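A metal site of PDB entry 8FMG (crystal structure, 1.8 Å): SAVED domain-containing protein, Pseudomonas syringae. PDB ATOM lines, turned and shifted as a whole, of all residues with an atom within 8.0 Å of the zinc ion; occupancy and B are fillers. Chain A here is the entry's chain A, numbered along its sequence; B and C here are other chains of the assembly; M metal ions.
SG of Cys 32 lies close to N of Leu 34, 3.5 Å away.
The side-chain sulfur (SG) of Cys 35 lies close to the backbone NH (N) of Thr 37, 3.7 Å away.
The backbone NH of Cys 32 sits at hydrogen-bond distance from the backbone carbonyl oxygen of Thr 37, 2.9 Å away.
The side-chain sulfur of Cys 87 sits close to the backbone NH of Gly 89, 3.8 Å away.
The nearest printed residue that does not touch the zinc ion is Thr 37 (4.5 Å).
The zinc ion is bound by SG of Cys 90, SG of Cys 32, SG of Cys 87 and SG of Cys 35.
The zinc ion has four donor atoms within binding distance.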
ATOM      1  N   HIS A  31      33.882  -4.096   4.530  1.00  0.00           N
ATOM      2  CA  HIS A  31      32.433  -4.125   4.415  1.00  0.00           C
ATOM      3  C   HIS A  31      31.808  -3.609   5.705  1.00  0.00           C
ATOM      4  O   HIS A  31      32.407  -3.703   6.783  1.00  0.00           O
ATOM      5  CB  HIS A  31      31.905  -5.538   4.137  1.00  0.00           C
ATOM      6  CG  HIS A  31      32.134  -6.014   2.737  1.00  0.00           C
ATOM      7  ND1 HIS A  31      33.396  -6.178   2.200  1.00  0.00           N
ATOM      8  CD2 HIS A  31      31.260  -6.385   1.776  1.00  0.00           C
ATOM      9  CE1 HIS A  31      33.288  -6.616   0.961  1.00  0.00           C
ATOM     10  NE2 HIS A  31      32.004  -6.754   0.673  1.00  0.00           N
ATOM     11  N   CYS A  32      30.598  -3.064   5.598  1.00  0.00           N
ATOM     12  CA  CYS A  32      29.877  -2.616   6.780  1.00  0.00           C
ATOM     13  C   CYS A  32      29.541  -3.819   7.648  1.00  0.00           C
ATOM     14  O   CYS A  32      28.941  -4.792   7.173  1.00  0.00           O
ATOM     15  CB  CYS A  32      28.615  -1.862   6.395  1.00  0.00           C
ATOM     16  SG  CYS A  32      27.632  -1.321   7.826  1.00  0.00           S
ATOM     17  N   GLU A  33      29.905  -3.751   8.928  1.00  0.00           N
ATOM     18  CA  GLU A  33      29.700  -4.880   9.817  1.00  0.00           C
ATOM     19  C   GLU A  33      28.225  -5.110  10.138  1.00  0.00           C
ATOM     20  O   GLU A  33      27.871  -6.191  10.612  1.00  0.00           O
ATOM     21  CB  GLU A  33      30.484  -4.685  11.114  1.00  0.00           C
ATOM     22  CG  GLU A  33      31.974  -4.577  10.902  1.00  0.00           C
ATOM     23  CD  GLU A  33      32.777  -4.473  12.183  1.00  0.00           C
ATOM     24  OE1 GLU A  33      32.347  -5.017  13.225  1.00  0.00           O
ATOM     25  OE2 GLU A  33      33.855  -3.832  12.158  1.00  0.00           O
ATOM     26  N   LEU A  34      27.365  -4.123   9.884  1.00  0.00           N
ATOM     27  CA  LEU A  34      25.959  -4.238  10.254  1.00  0.00           C
ATOM     28  C   LEU A  34      25.031  -4.513   9.078  1.00  0.00           C
ATOM     29  O   LEU A  34      23.947  -5.080   9.286  1.00  0.00           O
ATOM     30  CB  LEU A  34      25.488  -2.959  10.966  1.00  0.00           C
ATOM     31  CG  LEU A  34      26.025  -2.745  12.376  1.00  0.00           C
ATOM     32  CD1 LEU A  34      25.519  -1.425  12.945  1.00  0.00           C
ATOM     33  CD2 LEU A  34      25.648  -3.896  13.307  1.00  0.00           C
ATOM     34  N   CYS A  35      25.407  -4.122   7.858  1.00  0.00           N
ATOM     35  CA  CYS A  35      24.583  -4.382   6.680  1.00  0.00           C
ATOM     36  C   CYS A  35      25.340  -5.091   5.567  1.00  0.00           C
ATOM     37  O   CYS A  35      24.705  -5.487   4.572  1.00  0.00           O
ATOM     38  CB  CYS A  35      23.989  -3.077   6.131  1.00  0.00           C
ATOM     39  SG  CYS A  35      25.121  -2.003   5.203  1.00  0.00           S
ATOM     40  N   GLY A  36      26.646  -5.270   5.676  1.00  0.00           N
ATOM     41  CA  GLY A  36      27.368  -6.062   4.708  1.00  0.00           C
ATOM     42  C   GLY A  36      27.631  -5.409   3.380  1.00  0.00           C
ATOM     43  O   GLY A  36      28.104  -6.097   2.462  1.00  0.00           O
ATOM     44  N   THR A  37      27.356  -4.113   3.220  1.00  0.00           N
ATOM     45  CA  THR A  37      27.649  -3.470   1.945  1.00  0.00           C
ATOM     46  C   THR A  37      29.152  -3.262   1.791  1.00  0.00           C
ATOM     47  O   THR A  37      29.882  -3.067   2.767  1.00  0.00           O
ATOM     48  CB  THR A  37      26.884  -2.145   1.805  1.00  0.00           C
ATOM     49  OG1 THR A  37      26.927  -1.717   0.440  1.00  0.00           O
ATOM     50  CG2 THR A  37      27.463  -1.061   2.686  1.00  0.00           C
ATOM     51  N   ASP A  38      29.608  -3.335   0.546  1.00  0.00           N
ATOM     52  CA  ASP A  38      31.017  -3.186   0.213  1.00  0.00           C
ATOM     53  C   ASP A  38      31.382  -1.700   0.240  1.00  0.00           C
ATOM     54  O   ASP A  38      30.838  -0.915  -0.526  1.00  0.00           O
ATOM     55  CB  ASP A  38      31.278  -3.808  -1.162  1.00  0.00           C
ATOM     56  CG  ASP A  38      32.725  -3.663  -1.614  1.00  0.00           C
ATOM     57  OD1 ASP A  38      33.528  -3.031  -0.895  1.00  0.00           O
ATOM     58  OD2 ASP A  38      33.035  -4.190  -2.698  1.00  0.00           O
ATOM     59  N   LEU A  39      32.318  -1.347   1.119  1.00  0.00           N
ATOM     60  CA  LEU A  39      32.692   0.039   1.346  1.00  0.00           C
ATOM     61  C   LEU A  39      33.962   0.450   0.615  1.00  0.00           C
ATOM     62  O   LEU A  39      34.472   1.548   0.847  1.00  0.00           O
ATOM     63  CB  LEU A  39      32.849   0.294   2.846  1.00  0.00           C
ATOM     64  CG  LEU A  39      31.580   0.144   3.681  1.00  0.00           C
ATOM     65  CD1 LEU A  39      31.909   0.139   5.168  1.00  0.00           C
ATOM     66  CD2 LEU A  39      30.597   1.258   3.377  1.00  0.00           C
ATOM     67  N   TRP A  51      34.392   4.671   1.248  1.00  0.00           N
ATOM     68  CA  TRP A  51      33.258   5.449   1.735  1.00  0.00           C
ATOM     69  C   TRP A  51      32.705   4.912   3.051  1.00  0.00           C
ATOM     70  O   TRP A  51      31.535   5.130   3.365  1.00  0.00           O
ATOM     71  CB  TRP A  51      32.173   5.541   0.656  1.00  0.00           C
ATOM     72  CG  TRP A  51      31.488   4.282   0.248  1.00  0.00           C
ATOM     73  CD1 TRP A  51      31.968   3.310  -0.582  1.00  0.00           C
ATOM     74  CD2 TRP A  51      30.164   3.867   0.619  1.00  0.00           C
ATOM     75  NE1 TRP A  51      31.036   2.320  -0.738  1.00  0.00           N
ATOM     76  CE2 TRP A  51      29.918   2.631  -0.011  1.00  0.00           C
ATOM     77  CE3 TRP A  51      29.169   4.416   1.429  1.00  0.00           C
ATOM     78  CZ2 TRP A  51      28.725   1.938   0.140  1.00  0.00           C
ATOM     79  CZ3 TRP A  51      27.985   3.730   1.582  1.00  0.00           C
ATOM     80  CH2 TRP A  51      27.773   2.501   0.945  1.00  0.00           C
ATOM     81  N   LEU A  85      33.741  -0.960  11.480  1.00  0.00           N
ATOM     82  CA  LEU A  85      33.642  -0.317  10.175  1.00  0.00           C
ATOM     83  C   LEU A  85      32.184  -0.315   9.766  1.00  0.00           C
ATOM     84  O   LEU A  85      31.586  -1.382   9.549  1.00  0.00           O
ATOM     85  CB  LEU A  85      34.496  -1.033   9.134  1.00  0.00           C
ATOM     86  CG  LEU A  85      34.575  -0.260   7.809  1.00  0.00           C
ATOM     87  CD1 LEU A  85      35.494   0.949   7.965  1.00  0.00           C
ATOM     88  CD2 LEU A  85      35.047  -1.147   6.682  1.00  0.00           C
ATOM     89  N   LEU A  86      31.603   0.877   9.655  1.00  0.00           N
ATOM     90  CA  LEU A  86      30.207   1.042   9.288  1.00  0.00           C
ATOM     91  C   LEU A  86      30.099   1.893   8.032  1.00  0.00           C
ATOM     92  O   LEU A  86      30.901   2.801   7.809  1.00  0.00           O
ATOM     93  CB  LEU A  86      29.414   1.707  10.416  1.00  0.00           C
ATOM     94  CG  LEU A  86      29.492   1.000  11.770  1.00  0.00           C
ATOM     95  CD1 LEU A  86      28.628   1.684  12.796  1.00  0.00           C
ATOM     96  CD2 LEU A  86      29.078  -0.446  11.605  1.00  0.00           C
ATOM     97  N   CYS A  87      29.098   1.592   7.213  1.00  0.00           N
ATOM     98  CA  CYS A  87      28.695   2.522   6.177  1.00  0.00           C
ATOM     99  C   CYS A  87      28.170   3.782   6.863  1.00  0.00           C
ATOM    100  O   CYS A  87      27.786   3.749   8.031  1.00  0.00           O
ATOM    101  CB  CYS A  87      27.654   1.922   5.260  1.00  0.00           C
ATOM    102  SG  CYS A  87      26.025   1.742   5.984  1.00  0.00           S
ATOM    103  N   PRO A  88      28.147   4.912   6.152  1.00  0.00           N
ATOM    104  CA  PRO A  88      27.739   6.163   6.802  1.00  0.00           C
ATOM    105  C   PRO A  88      26.329   6.129   7.377  1.00  0.00           C
ATOM    106  O   PRO A  88      26.077   6.738   8.415  1.00  0.00           O
ATOM    107  CB  PRO A  88      27.871   7.209   5.681  1.00  0.00           C
ATOM    108  CG  PRO A  88      28.875   6.626   4.748  1.00  0.00           C
ATOM    109  CD  PRO A  88      28.623   5.137   4.773  1.00  0.00           C
ATOM    110  N   GLY A  89      25.413   5.419   6.720  1.00  0.00           N
ATOM    111  CA  GLY A  89      24.047   5.373   7.212  1.00  0.00           C
ATOM    112  C   GLY A  89      23.908   4.561   8.490  1.00  0.00           C
ATOM    113  O   GLY A  89      23.261   4.997   9.446  1.00  0.00           O
ATOM    114  N   CYS A  90      24.494   3.363   8.513  1.00  0.00           N
ATOM    115  CA  CYS A  90      24.443   2.559   9.725  1.00  0.00           C
ATOM    116  C   CYS A  90      25.060   3.318  10.903  1.00  0.00           C
ATOM    117  O   CYS A  90      24.505   3.307  12.007  1.00  0.00           O
ATOM    118  CB  CYS A  90      25.128   1.211   9.513  1.00  0.00           C
ATOM    119  SG  CYS A  90      24.206   0.056   8.434  1.00  0.00           S
ATOM    120  N   HIS A  91      26.188   4.006  10.683  1.00  0.00           N
ATOM    121  CA  HIS A  91      26.785   4.776  11.772  1.00  0.00           C
ATOM    122  C   HIS A  91      25.845   5.869  12.265  1.00  0.00           C
ATOM    123  O   HIS A  91      25.698   6.072  13.475  1.00  0.00           O
ATOM    124  CB  HIS A  91      28.115   5.395  11.327  1.00  0.00           C
ATOM    125  CG  HIS A  91      28.853   6.100  12.432  1.00  0.00           C
ATOM    126  ND1 HIS A  91      29.991   6.847  12.211  1.00  0.00           N
ATOM    127  CD2 HIS A  91      28.615   6.165  13.767  1.00  0.00           C
ATOM    128  CE1 HIS A  91      30.409   7.343  13.362  1.00  0.00           C
ATOM    129  NE2 HIS A  91      29.603   6.947  14.312  1.00  0.00           N
ATOM    130  N   LYS A  93      22.641   5.852  12.216  1.00  0.00           N
ATOM    131  CA  LYS A  93      21.491   5.286  12.903  1.00  0.00           C
ATOM    132  C   LYS A  93      21.833   4.826  14.312  1.00  0.00           C
ATOM    133  O   LYS A  93      21.062   5.052  15.250  1.00  0.00           O
ATOM    134  CB  LYS A  93      20.925   4.117  12.094  1.00  0.00           C
ATOM    135  CG  LYS A  93      20.267   4.523  10.779  1.00  0.00           C
ATOM    136  CD  LYS A  93      19.929   3.272   9.987  1.00  0.00           C
ATOM    137  CE  LYS A  93      19.528   3.603   8.572  1.00  0.00           C
ATOM    138  NZ  LYS A  93      19.389   2.357   7.767  1.00  0.00           N
ATOM    139  N   ARG B  44      15.279  -0.804  11.054  1.00  0.00           N
ATOM    140  CA  ARG B  44      15.927  -1.910  11.754  1.00  0.00           C
ATOM    141  C   ARG B  44      15.539  -1.941  13.230  1.00  0.00           C
ATOM    142  O   ARG B  44      15.189  -2.999  13.761  1.00  0.00           O
ATOM    143  CB  ARG B  44      17.447  -1.822  11.615  1.00  0.00           C
ATOM    144  CG  ARG B  44      18.161  -2.845  12.489  1.00  0.00           C
ATOM    145  CD  ARG B  44      19.605  -3.056  12.080  1.00  0.00           C
ATOM    146  NE  ARG B  44      20.230  -4.079  12.918  1.00  0.00           N
ATOM    147  CZ  ARG B  44      21.370  -4.697  12.627  1.00  0.00           C
ATOM    148  NH1 ARG B  44      22.048  -4.414  11.532  1.00  0.00           N
ATOM    149  NH2 ARG B  44      21.829  -5.636  13.450  1.00  0.00           N
ATOM    150  N   PRO C 124      26.068 -10.000   6.827  1.00  0.00           N
ATOM    151  CA  PRO C 124      25.001  -9.197   7.453  1.00  0.00           C
ATOM    152  C   PRO C 124      23.764  -9.034   6.592  1.00  0.00           C
ATOM    153  O   PRO C 124      22.657  -8.916   7.143  1.00  0.00           O
ATOM    154  CB  PRO C 124      25.694  -7.856   7.726  1.00  0.00           C
ATOM    155  CG  PRO C 124      27.129  -8.232   7.945  1.00  0.00           C
ATOM    156  CD  PRO C 124      27.392  -9.345   6.952  1.00  0.00           C
HETATM  157 ZN    ZN M   1      25.763  -0.425   6.788  1.00  0.00          ZN
